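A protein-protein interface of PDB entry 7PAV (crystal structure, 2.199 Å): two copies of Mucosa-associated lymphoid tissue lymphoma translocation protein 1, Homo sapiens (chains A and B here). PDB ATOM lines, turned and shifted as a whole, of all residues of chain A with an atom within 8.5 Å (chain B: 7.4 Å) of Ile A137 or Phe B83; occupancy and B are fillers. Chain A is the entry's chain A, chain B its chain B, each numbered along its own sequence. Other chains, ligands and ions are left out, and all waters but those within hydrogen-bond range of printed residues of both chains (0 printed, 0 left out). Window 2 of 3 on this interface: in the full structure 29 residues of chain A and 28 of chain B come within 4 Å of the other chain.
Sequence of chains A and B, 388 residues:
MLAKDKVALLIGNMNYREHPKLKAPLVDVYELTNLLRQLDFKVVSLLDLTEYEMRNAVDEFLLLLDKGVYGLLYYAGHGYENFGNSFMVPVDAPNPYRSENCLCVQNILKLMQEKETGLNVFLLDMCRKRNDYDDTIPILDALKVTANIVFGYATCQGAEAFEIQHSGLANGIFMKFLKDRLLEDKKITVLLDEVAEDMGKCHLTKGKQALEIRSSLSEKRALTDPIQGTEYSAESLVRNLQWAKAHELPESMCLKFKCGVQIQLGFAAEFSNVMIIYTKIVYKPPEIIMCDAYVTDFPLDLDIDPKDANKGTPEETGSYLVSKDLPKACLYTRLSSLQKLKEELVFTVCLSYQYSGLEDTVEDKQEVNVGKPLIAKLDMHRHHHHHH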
ATOM      1  N   GLU A  81     -18.019  -2.798 -14.961  1.00  0.00           N
ATOM      2  CA  GLU A  81     -17.426  -2.742 -13.648  1.00  0.00           C
ATOM      3  C   GLU A  81     -18.028  -3.744 -12.707  1.00  0.00           C
ATOM      4  O   GLU A  81     -19.201  -3.639 -12.371  1.00  0.00           O
ATOM      5  CB  GLU A  81     -17.492  -1.338 -13.093  1.00  0.00           C
ATOM      6  CG  GLU A  81     -16.581  -1.175 -11.895  1.00  0.00           C
ATOM      7  CD  GLU A  81     -16.507   0.262 -11.446  1.00  0.00           C
ATOM      8  OE1 GLU A  81     -16.122   1.121 -12.276  1.00  0.00           O
ATOM      9  OE2 GLU A  81     -16.866   0.531 -10.277  1.00  0.00           O
ATOM     10  N   ASN A  82     -17.225  -4.730 -12.275  1.00  0.00           N
ATOM     11  CA  ASN A  82     -17.679  -5.779 -11.364  1.00  0.00           C
ATOM     12  C   ASN A  82     -16.810  -5.798 -10.142  1.00  0.00           C
ATOM     13  O   ASN A  82     -15.583  -5.786 -10.278  1.00  0.00           O
ATOM     14  CB  ASN A  82     -17.616  -7.171 -12.009  1.00  0.00           C
ATOM     15  CG  ASN A  82     -18.820  -7.530 -12.825  1.00  0.00           C
ATOM     16  OD1 ASN A  82     -19.438  -6.684 -13.458  1.00  0.00           O
ATOM     17  ND2 ASN A  82     -19.157  -8.797 -12.855  1.00  0.00           N
ATOM     18  N   PHE A  83     -17.434  -5.838  -8.954  1.00  0.00           N
ATOM     19  CA  PHE A  83     -16.763  -5.920  -7.660  1.00  0.00           C
ATOM     20  C   PHE A  83     -15.583  -4.954  -7.495  1.00  0.00           C
ATOM     21  O   PHE A  83     -14.509  -5.358  -7.059  1.00  0.00           O
ATOM     22  CB  PHE A  83     -16.339  -7.359  -7.369  1.00  0.00           C
ATOM     23  CG  PHE A  83     -17.480  -8.326  -7.524  1.00  0.00           C
ATOM     24  CD1 PHE A  83     -18.595  -8.243  -6.708  1.00  0.00           C
ATOM     25  CD2 PHE A  83     -17.463  -9.288  -8.519  1.00  0.00           C
ATOM     26  CE1 PHE A  83     -19.655  -9.134  -6.861  1.00  0.00           C
ATOM     27  CE2 PHE A  83     -18.521 -10.177  -8.663  1.00  0.00           C
ATOM     28  CZ  PHE A  83     -19.610 -10.091  -7.838  1.00  0.00           C
ATOM     29  N   GLY A  84     -15.788  -3.705  -7.905  1.00  0.00           N
ATOM     30  CA  GLY A  84     -14.780  -2.669  -7.778  1.00  0.00           C
ATOM     31  C   GLY A  84     -13.822  -2.549  -8.936  1.00  0.00           C
ATOM     32  O   GLY A  84     -13.135  -1.531  -9.051  1.00  0.00           O
ATOM     33  N   ASN A  85     -13.764  -3.567  -9.808  1.00  0.00           N
ATOM     34  CA  ASN A  85     -12.830  -3.588 -10.931  1.00  0.00           C
ATOM     35  C   ASN A  85     -13.446  -3.221 -12.292  1.00  0.00           C
ATOM     36  O   ASN A  85     -14.544  -3.660 -12.622  1.00  0.00           O
ATOM     37  CB  ASN A  85     -12.165  -4.959 -11.029  1.00  0.00           C
ATOM     38  CG  ASN A  85     -11.319  -5.309  -9.845  1.00  0.00           C
ATOM     39  OD1 ASN A  85     -11.455  -6.388  -9.265  1.00  0.00           O
ATOM     40  ND2 ASN A  85     -10.441  -4.402  -9.445  1.00  0.00           N
ATOM     41  N   PHE A  87     -13.351  -3.447 -16.459  1.00  0.00           N
ATOM     42  CA  PHE A  87     -12.873  -4.281 -17.545  1.00  0.00           C
ATOM     43  C   PHE A  87     -13.067  -3.613 -18.904  1.00  0.00           C
ATOM     44  O   PHE A  87     -14.064  -2.936 -19.159  1.00  0.00           O
ATOM     45  CB  PHE A  87     -13.511  -5.671 -17.493  1.00  0.00           C
ATOM     46  CG  PHE A  87     -13.283  -6.402 -16.190  1.00  0.00           C
ATOM     47  CD1 PHE A  87     -14.029  -6.093 -15.060  1.00  0.00           C
ATOM     48  CD2 PHE A  87     -12.321  -7.396 -16.093  1.00  0.00           C
ATOM     49  CE1 PHE A  87     -13.792  -6.736 -13.856  1.00  0.00           C
ATOM     50  CE2 PHE A  87     -12.100  -8.055 -14.887  1.00  0.00           C
ATOM     51  CZ  PHE A  87     -12.831  -7.714 -13.775  1.00  0.00           C
ATOM     52  N   ARG A  98     -16.889 -12.865 -20.574  1.00  0.00           N
ATOM     53  CA  ARG A  98     -16.478 -12.959 -19.180  1.00  0.00           C
ATOM     54  C   ARG A  98     -15.175 -12.167 -18.962  1.00  0.00           C
ATOM     55  O   ARG A  98     -14.671 -11.553 -19.899  1.00  0.00           O
ATOM     56  CB  ARG A  98     -16.303 -14.441 -18.799  1.00  0.00           C
ATOM     57  CG  ARG A  98     -17.579 -15.275 -18.771  1.00  0.00           C
ATOM     58  CD  ARG A  98     -17.282 -16.748 -18.502  1.00  0.00           C
ATOM     59  NE  ARG A  98     -16.326 -16.921 -17.402  1.00  0.00           N
ATOM     60  CZ  ARG A  98     -16.650 -17.305 -16.170  1.00  0.00           C
ATOM     61  NH1 ARG A  98     -17.907 -17.613 -15.871  1.00  0.00           N
ATOM     62  NH2 ARG A  98     -15.713 -17.411 -15.237  1.00  0.00           N
ATOM     63  N   SER A  99     -14.633 -12.173 -17.718  1.00  0.00           N
ATOM     64  CA  SER A  99     -13.409 -11.446 -17.339  1.00  0.00           C
ATOM     65  C   SER A  99     -12.179 -11.939 -18.092  1.00  0.00           C
ATOM     66  O   SER A  99     -11.291 -11.146 -18.393  1.00  0.00           O
ATOM     67  CB  SER A  99     -13.176 -11.535 -15.830  1.00  0.00           C
ATOM     68  OG  SER A  99     -12.860 -12.860 -15.445  1.00  0.00           O
ATOM     69  N   ARG A 130     -22.591  -3.530 -14.236  1.00  0.00           N
ATOM     70  CA  ARG A 130     -22.175  -4.908 -14.022  1.00  0.00           C
ATOM     71  C   ARG A 130     -22.409  -5.759 -15.274  1.00  0.00           C
ATOM     72  O   ARG A 130     -23.369  -5.542 -16.017  1.00  0.00           O
ATOM     73  CB  ARG A 130     -22.978  -5.519 -12.854  1.00  0.00           C
ATOM     74  CG  ARG A 130     -22.117  -5.867 -11.652  1.00  0.00           C
ATOM     75  CD  ARG A 130     -22.811  -6.705 -10.582  1.00  0.00           C
ATOM     76  NE  ARG A 130     -22.097  -7.965 -10.333  1.00  0.00           N
ATOM     77  CZ  ARG A 130     -22.286  -9.077 -11.045  1.00  0.00           C
ATOM     78  NH1 ARG A 130     -23.127  -9.082 -12.068  1.00  0.00           N
ATOM     79  NH2 ARG A 130     -21.612 -10.185 -10.755  1.00  0.00           N
ATOM     80  N   ASP A 134     -20.440 -12.492 -15.660  1.00  0.00           N
ATOM     81  CA  ASP A 134     -19.140 -12.678 -15.038  1.00  0.00           C
ATOM     82  C   ASP A 134     -19.273 -13.086 -13.550  1.00  0.00           C
ATOM     83  O   ASP A 134     -19.398 -12.227 -12.667  1.00  0.00           O
ATOM     84  CB  ASP A 134     -18.315 -11.394 -15.188  1.00  0.00           C
ATOM     85  CG  ASP A 134     -16.875 -11.573 -14.796  1.00  0.00           C
ATOM     86  OD1 ASP A 134     -16.347 -12.690 -14.990  1.00  0.00           O
ATOM     87  OD2 ASP A 134     -16.268 -10.595 -14.301  1.00  0.00           O
ATOM     88  N   ASP A 135     -19.238 -14.406 -13.284  1.00  0.00           N
ATOM     89  CA  ASP A 135     -19.335 -14.977 -11.928  1.00  0.00           C
ATOM     90  C   ASP A 135     -18.045 -14.875 -11.104  1.00  0.00           C
ATOM     91  O   ASP A 135     -18.031 -15.284  -9.944  1.00  0.00           O
ATOM     92  CB  ASP A 135     -19.716 -16.471 -12.010  1.00  0.00           C
ATOM     93  CG  ASP A 135     -21.094 -16.758 -12.567  1.00  0.00           C
ATOM     94  OD1 ASP A 135     -21.771 -15.797 -13.001  1.00  0.00           O
ATOM     95  OD2 ASP A 135     -21.500 -17.946 -12.570  1.00  0.00           O
ATOM     96  N   THR A 136     -16.966 -14.386 -11.708  1.00  0.00           N
ATOM     97  CA  THR A 136     -15.636 -14.289 -11.123  1.00  0.00           C
ATOM     98  C   THR A 136     -15.524 -13.284  -9.966  1.00  0.00           C
ATOM     99  O   THR A 136     -15.834 -12.106 -10.132  1.00  0.00           O
ATOM    100  CB  THR A 136     -14.644 -13.979 -12.247  1.00  0.00           C
ATOM    101  OG1 THR A 136     -14.820 -14.930 -13.302  1.00  0.00           O
ATOM    102  CG2 THR A 136     -13.203 -13.960 -11.777  1.00  0.00           C
ATOM    103  N   ILE A 137     -15.054 -13.753  -8.802  1.00  0.00           N
ATOM    104  CA  ILE A 137     -14.847 -12.911  -7.624  1.00  0.00           C
ATOM    105  C   ILE A 137     -13.344 -12.574  -7.598  1.00  0.00           C
ATOM    106  O   ILE A 137     -12.532 -13.493  -7.519  1.00  0.00           O
ATOM    107  CB  ILE A 137     -15.270 -13.587  -6.275  1.00  0.00           C
ATOM    108  CG1 ILE A 137     -16.261 -14.782  -6.434  1.00  0.00           C
ATOM    109  CG2 ILE A 137     -15.812 -12.563  -5.291  1.00  0.00           C
ATOM    110  CD1 ILE A 137     -17.777 -14.458  -6.586  1.00  0.00           C
ATOM    111  N   PRO A 138     -12.942 -11.287  -7.664  1.00  0.00           N
ATOM    112  CA  PRO A 138     -11.501 -10.955  -7.635  1.00  0.00           C
ATOM    113  C   PRO A 138     -10.743 -11.561  -6.451  1.00  0.00           C
ATOM    114  O   PRO A 138     -11.323 -11.761  -5.384  1.00  0.00           O
ATOM    115  CB  PRO A 138     -11.488  -9.426  -7.587  1.00  0.00           C
ATOM    116  CG  PRO A 138     -12.800  -9.016  -8.127  1.00  0.00           C
ATOM    117  CD  PRO A 138     -13.777 -10.076  -7.758  1.00  0.00           C
ATOM    118  N   ILE A 139      -9.457 -11.889  -6.649  1.00  0.00           N
ATOM    119  CA  ILE A 139      -8.627 -12.548  -5.635  1.00  0.00           C
ATOM    120  C   ILE A 139      -8.573 -11.735  -4.322  1.00  0.00           C
ATOM    121  O   ILE A 139      -9.182 -12.175  -3.339  1.00  0.00           O
ATOM    122  CB  ILE A 139      -7.225 -12.950  -6.183  1.00  0.00           C
ATOM    123  CG1 ILE A 139      -7.347 -13.899  -7.388  1.00  0.00           C
ATOM    124  CG2 ILE A 139      -6.341 -13.540  -5.102  1.00  0.00           C
ATOM    125  CD1 ILE A 139      -7.345 -13.172  -8.758  1.00  0.00           C
ATOM    126  N   LEU A 140      -7.984 -10.524  -4.289  1.00  0.00           N
ATOM    127  CA  LEU A 140      -7.161  -9.838  -5.292  1.00  0.00           C
ATOM    128  C   LEU A 140      -5.850  -9.414  -4.594  1.00  0.00           C
ATOM    129  O   LEU A 140      -5.787  -9.375  -3.352  1.00  0.00           O
ATOM    130  CB  LEU A 140      -7.891  -8.617  -5.865  1.00  0.00           C
ATOM    131  N   GLN A 157     -20.641   5.017 -11.046  1.00  0.00           N
ATOM    132  CA  GLN A 157     -20.749   3.567 -10.923  1.00  0.00           C
ATOM    133  C   GLN A 157     -22.181   3.110 -11.101  1.00  0.00           C
ATOM    134  O   GLN A 157     -23.074   3.687 -10.499  1.00  0.00           O
ATOM    135  CB  GLN A 157     -20.221   3.154  -9.548  1.00  0.00           C
ATOM    136  CG  GLN A 157     -20.063   1.659  -9.347  1.00  0.00           C
ATOM    137  CD  GLN A 157     -19.320   1.383  -8.062  1.00  0.00           C
ATOM    138  OE1 GLN A 157     -18.402   2.127  -7.667  1.00  0.00           O
ATOM    139  NE2 GLN A 157     -19.691   0.298  -7.390  1.00  0.00           N
ATOM    140  N   GLU B  81     -12.990  -3.385   3.937  1.00  0.00           N
ATOM    141  CA  GLU B  81     -13.452  -3.135   2.578  1.00  0.00           C
ATOM    142  C   GLU B  81     -13.448  -4.414   1.803  1.00  0.00           C
ATOM    143  O   GLU B  81     -12.402  -5.034   1.615  1.00  0.00           O
ATOM    144  CB  GLU B  81     -12.573  -2.113   1.862  1.00  0.00           C
ATOM    145  CG  GLU B  81     -13.081  -1.757   0.481  1.00  0.00           C
ATOM    146  CD  GLU B  81     -13.095  -0.264   0.244  1.00  0.00           C
ATOM    147  OE1 GLU B  81     -13.570   0.474   1.137  1.00  0.00           O
ATOM    148  OE2 GLU B  81     -12.620   0.176  -0.825  1.00  0.00           O
ATOM    149  N   ASN B  82     -14.630  -4.826   1.364  1.00  0.00           N
ATOM    150  CA  ASN B  82     -14.778  -6.036   0.584  1.00  0.00           C
ATOM    151  C   ASN B  82     -15.440  -5.705  -0.748  1.00  0.00           C
ATOM    152  O   ASN B  82     -16.582  -5.218  -0.770  1.00  0.00           O
ATOM    153  CB  ASN B  82     -15.630  -7.062   1.335  1.00  0.00           C
ATOM    154  CG  ASN B  82     -14.840  -7.895   2.283  1.00  0.00           C
ATOM    155  OD1 ASN B  82     -13.842  -7.449   2.830  1.00  0.00           O
ATOM    156  ND2 ASN B  82     -15.242  -9.129   2.485  1.00  0.00           N
ATOM    157  N   PHE B  83     -14.694  -5.919  -1.841  1.00  0.00           N
ATOM    158  CA  PHE B  83     -15.153  -5.769  -3.225  1.00  0.00           C
ATOM    159  C   PHE B  83     -15.791  -4.418  -3.529  1.00  0.00           C
ATOM    160  O   PHE B  83     -16.834  -4.344  -4.169  1.00  0.00           O
ATOM    161  CB  PHE B  83     -16.086  -6.923  -3.569  1.00  0.00           C
ATOM    162  CG  PHE B  83     -15.376  -8.246  -3.390  1.00  0.00           C
ATOM    163  CD1 PHE B  83     -14.391  -8.644  -4.270  1.00  0.00           C
ATOM    164  CD2 PHE B  83     -15.652  -9.058  -2.303  1.00  0.00           C
ATOM    165  CE1 PHE B  83     -13.727  -9.846  -4.096  1.00  0.00           C
ATOM    166  CE2 PHE B  83     -14.960 -10.242  -2.108  1.00  0.00           C
ATOM    167  CZ  PHE B  83     -13.994 -10.628  -3.000  1.00  0.00           C
ATOM    168  N   GLY B  84     -15.168  -3.367  -3.023  1.00  0.00           N
ATOM    169  CA  GLY B  84     -15.649  -2.015  -3.222  1.00  0.00           C
ATOM    170  C   GLY B  84     -16.427  -1.473  -2.054  1.00  0.00           C
ATOM    171  O   GLY B  84     -16.405  -0.267  -1.807  1.00  0.00           O
ATOM    172  N   ASN B  85     -17.103  -2.362  -1.307  1.00  0.00           N
ATOM    173  CA  ASN B  85     -17.980  -1.984  -0.196  1.00  0.00           C
ATOM    174  C   ASN B  85     -17.273  -1.798   1.134  1.00  0.00           C
ATOM    175  O   ASN B  85     -16.485  -2.659   1.516  1.00  0.00           O
ATOM    176  CB  ASN B  85     -19.088  -3.033  -0.064  1.00  0.00           C
ATOM    177  CG  ASN B  85     -19.933  -3.138  -1.311  1.00  0.00           C
ATOM    178  OD1 ASN B  85     -20.157  -4.224  -1.844  1.00  0.00           O
ATOM    179  ND2 ASN B  85     -20.410  -1.987  -1.804  1.00  0.00           N
ATOM    180  N   SER B  86     -17.586  -0.703   1.859  1.00  0.00           N
ATOM    181  CA  SER B  86     -16.979  -0.414   3.153  1.00  0.00           C
ATOM    182  C   SER B  86     -17.908  -0.808   4.287  1.00  0.00           C
ATOM    183  O   SER B  86     -19.110  -0.570   4.196  1.00  0.00           O
ATOM    184  CB  SER B  86     -16.656   1.077   3.289  1.00  0.00           C
ATOM    185  OG  SER B  86     -15.683   1.529   2.360  1.00  0.00           O
ATOM    186  N   PHE B  87     -17.357  -1.366   5.371  1.00  0.00           N
ATOM    187  CA  PHE B  87     -18.175  -1.727   6.530  1.00  0.00           C
ATOM    188  C   PHE B  87     -17.619  -1.184   7.828  1.00  0.00           C
ATOM    189  O   PHE B  87     -16.426  -1.267   8.072  1.00  0.00           O
ATOM    190  CB  PHE B  87     -18.365  -3.232   6.639  1.00  0.00           C
ATOM    191  CG  PHE B  87     -19.011  -3.870   5.442  1.00  0.00           C
ATOM    192  CD1 PHE B  87     -18.249  -4.294   4.369  1.00  0.00           C
ATOM    193  CD2 PHE B  87     -20.371  -4.109   5.418  1.00  0.00           C
ATOM    194  CE1 PHE B  87     -18.836  -4.914   3.294  1.00  0.00           C
ATOM    195  CE2 PHE B  87     -20.956  -4.715   4.331  1.00  0.00           C
ATOM    196  CZ  PHE B  87     -20.189  -5.111   3.272  1.00  0.00           C
ATOM    197  N   ARG B 130      -9.459  -6.565   3.270  1.00  0.00           N
ATOM    198  CA  ARG B 130     -10.522  -7.536   3.056  1.00  0.00           C
ATOM    199  C   ARG B 130     -10.801  -8.324   4.330  1.00  0.00           C
ATOM    200  O   ARG B 130      -9.897  -8.554   5.142  1.00  0.00           O
ATOM    201  CB  ARG B 130     -10.146  -8.499   1.904  1.00  0.00           C
ATOM    202  CG  ARG B 130     -11.349  -9.205   1.254  1.00  0.00           C
ATOM    203  CD  ARG B 130     -11.075  -9.892  -0.096  1.00  0.00           C
ATOM    204  NE  ARG B 130      -9.776 -10.568  -0.158  1.00  0.00           N
ATOM    205  CZ  ARG B 130      -9.498 -11.728   0.436  1.00  0.00           C
ATOM    206  NH1 ARG B 130     -10.423 -12.352   1.160  1.00  0.00           N
ATOM    207  NH2 ARG B 130      -8.283 -12.258   0.336  1.00  0.00           N
ATOM    208  N   ASN B 131     -12.055  -8.724   4.508  1.00  0.00           N
ATOM    209  CA  ASN B 131     -12.476  -9.560   5.619  1.00  0.00           C
ATOM    210  C   ASN B 131     -12.698 -10.960   5.036  1.00  0.00           C
ATOM    211  O   ASN B 131     -13.709 -11.203   4.375  1.00  0.00           O
ATOM    212  CB  ASN B 131     -13.756  -9.013   6.261  1.00  0.00           C
ATOM    213  CG  ASN B 131     -14.432  -9.909   7.279  1.00  0.00           C
ATOM    214  OD1 ASN B 131     -13.885 -10.936   7.711  1.00  0.00           O
ATOM    215  ND2 ASN B 131     -15.648  -9.547   7.673  1.00  0.00           N
ATOM    216  N   ASP B 134     -16.292 -12.915   5.368  1.00  0.00           N
ATOM    217  CA  ASP B 134     -17.535 -12.493   4.751  1.00  0.00           C
ATOM    218  C   ASP B 134     -17.912 -13.311   3.522  1.00  0.00           C
ATOM    219  O   ASP B 134     -17.461 -12.992   2.422  1.00  0.00           O
ATOM    220  CB  ASP B 134     -17.471 -11.005   4.423  1.00  0.00           C
ATOM    221  CG  ASP B 134     -18.798 -10.289   4.536  1.00  0.00           C
ATOM    222  OD1 ASP B 134     -19.712 -10.828   5.210  1.00  0.00           O
ATOM    223  OD2 ASP B 134     -18.922  -9.174   3.970  1.00  0.00           O
ATOM    224  N   ASP B 135     -18.771 -14.340   3.711  1.00  0.00           N
ATOM    225  CA  ASP B 135     -19.262 -15.259   2.665  1.00  0.00           C
ATOM    226  C   ASP B 135     -20.066 -14.493   1.606  1.00  0.00           C
ATOM    227  O   ASP B 135     -19.966 -14.806   0.419  1.00  0.00           O
ATOM    228  CB  ASP B 135     -20.120 -16.382   3.304  1.00  0.00           C
ATOM    229  CG  ASP B 135     -20.732 -17.424   2.369  1.00  0.00           C
ATOM    230  OD1 ASP B 135     -20.828 -17.155   1.144  1.00  0.00           O
ATOM    231  OD2 ASP B 135     -21.129 -18.517   2.865  1.00  0.00           O
ATOM    232  N   THR B 136     -20.862 -13.497   2.029  1.00  0.00           N
ATOM    233  CA  THR B 136     -21.672 -12.727   1.092  1.00  0.00           C
ATOM    234  C   THR B 136     -20.933 -11.558   0.510  1.00  0.00           C
ATOM    235  O   THR B 136     -20.122 -10.923   1.182  1.00  0.00           O
ATOM    236  CB  THR B 136     -22.982 -12.241   1.728  1.00  0.00           C
ATOM    237  OG1 THR B 136     -22.734 -11.712   3.036  1.00  0.00           O
ATOM    238  CG2 THR B 136     -24.031 -13.320   1.784  1.00  0.00           C
ATOM    239  N   ILE B 137     -21.235 -11.259  -0.750  1.00  0.00           N
ATOM    240  CA  ILE B 137     -20.704 -10.113  -1.471  1.00  0.00           C
ATOM    241  C   ILE B 137     -21.937  -9.362  -1.949  1.00  0.00           C
ATOM    242  O   ILE B 137     -22.570  -9.765  -2.926  1.00  0.00           O
ATOM    243  CB  ILE B 137     -19.780 -10.517  -2.645  1.00  0.00           C
ATOM    244  CG1 ILE B 137     -18.656 -11.467  -2.193  1.00  0.00           C
ATOM    245  CG2 ILE B 137     -19.203  -9.282  -3.304  1.00  0.00           C
ATOM    246  CD1 ILE B 137     -18.884 -12.963  -2.513  1.00  0.00           C
ATOM    247  N   PRO B 138     -22.365  -8.339  -1.199  1.00  0.00           N
ATOM    248  CA  PRO B 138     -23.588  -7.622  -1.580  1.00  0.00           C
ATOM    249  C   PRO B 138     -23.510  -6.873  -2.903  1.00  0.00           C
ATOM    250  O   PRO B 138     -22.567  -6.133  -3.174  1.00  0.00           O
ATOM    251  CB  PRO B 138     -23.828  -6.664  -0.405  1.00  0.00           C
ATOM    252  CG  PRO B 138     -22.495  -6.475   0.209  1.00  0.00           C
ATOM    253  CD  PRO B 138     -21.757  -7.773   0.021  1.00  0.00           C
ATOM    254  N   GLN B 157      -7.289   1.279  -0.592  1.00  0.00           N
ATOM    255  CA  GLN B 157      -7.869  -0.048  -0.529  1.00  0.00           C
ATOM    256  C   GLN B 157      -6.792  -1.104  -0.334  1.00  0.00           C
ATOM    257  O   GLN B 157      -5.740  -1.045  -0.979  1.00  0.00           O
ATOM    258  CB  GLN B 157      -8.649  -0.324  -1.812  1.00  0.00           C
ATOM    259  CG  GLN B 157      -9.643  -1.468  -1.688  1.00  0.00           C
ATOM    260  CD  GLN B 157     -10.691  -1.454  -2.790  1.00  0.00           C
ATOM    261  OE1 GLN B 157     -10.567  -0.750  -3.814  1.00  0.00           O
ATOM    262  NE2 GLN B 157     -11.767  -2.233  -2.585  1.00  0.00           N
ATOM    263  N   ARG B 214     -12.799   9.770  -3.468  1.00  0.00           N
ATOM    264  CA  ARG B 214     -13.691   9.329  -4.572  1.00  0.00           C
ATOM    265  C   ARG B 214     -14.799  10.356  -4.591  1.00  0.00           C
ATOM    266  O   ARG B 214     -15.470  10.564  -3.569  1.00  0.00           O
ATOM    267  CB  ARG B 214     -14.275   7.935  -4.371  1.00  0.00           C
ATOM    268  CG  ARG B 214     -13.221   6.877  -4.215  1.00  0.00           C
ATOM    269  CD  ARG B 214     -13.846   5.506  -4.326  1.00  0.00           C
ATOM    270  NE  ARG B 214     -12.902   4.423  -4.026  1.00  0.00           N
ATOM    271  CZ  ARG B 214     -13.262   3.156  -3.814  1.00  0.00           C
ATOM    272  NH1 ARG B 214     -14.544   2.808  -3.844  1.00  0.00           N
ATOM    273  NH2 ARG B 214     -12.346   2.235  -3.557  1.00  0.00           N
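Phe A83 touches Phe B83. Ile B137 touches Phe A83 (CG2 to CE1, 3.6 Å). Gly A84 touches Phe B83 (N to O, 3.9 Å). Ile A137 touches Phe B83. O of Pro A138 touches CE1 of Phe B83 (3.3 Å). O of Ile A139 touches NE of Arg B130, 3.6 Å away.
Ile A137 touches just one residue of chain B: Phe B83 (3.5 Å). Phe B83 touches just these residues of chain A: Phe A83 (3.6 Å), Gly A84 (3.9 Å), Ile A137 (3.5 Å) and Pro A138 (3.3 Å). Printed residues of chain B within 4 Å of Ile A139: Arg B130. Of the printed residues of chain B, Gly A84 touches Phe B83. Asp A135 touches none of the printed residues of chain B.
Of the 17 printed residues of chain A, 5 touch a printed residue of chain B. Hydrophobic or aromatic side chains of chain A that line the printed part of chain B: Phe A83, Ile A137 and Pro A138. Along chain A the printed residues that touch a printed residue of chain B span positions 83 to 139. Printed residues of chain B that touch a printed residue of chain A: Phe B83, Arg B130 and Ile B137.
Phe A83 touches its own counterpart, Phe B83. Phe A83 touches Ile B137, and with the chains exchanged Ile A137 touches Phe B83. Gly A84 touches Phe B83, but with the chains exchanged Phe A83 does not touch Gly B84 (4.5 Å). Pro A138 touches Phe B83, but with the chains exchanged Phe A83 does not touch Pro B138 (5.6 Å).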
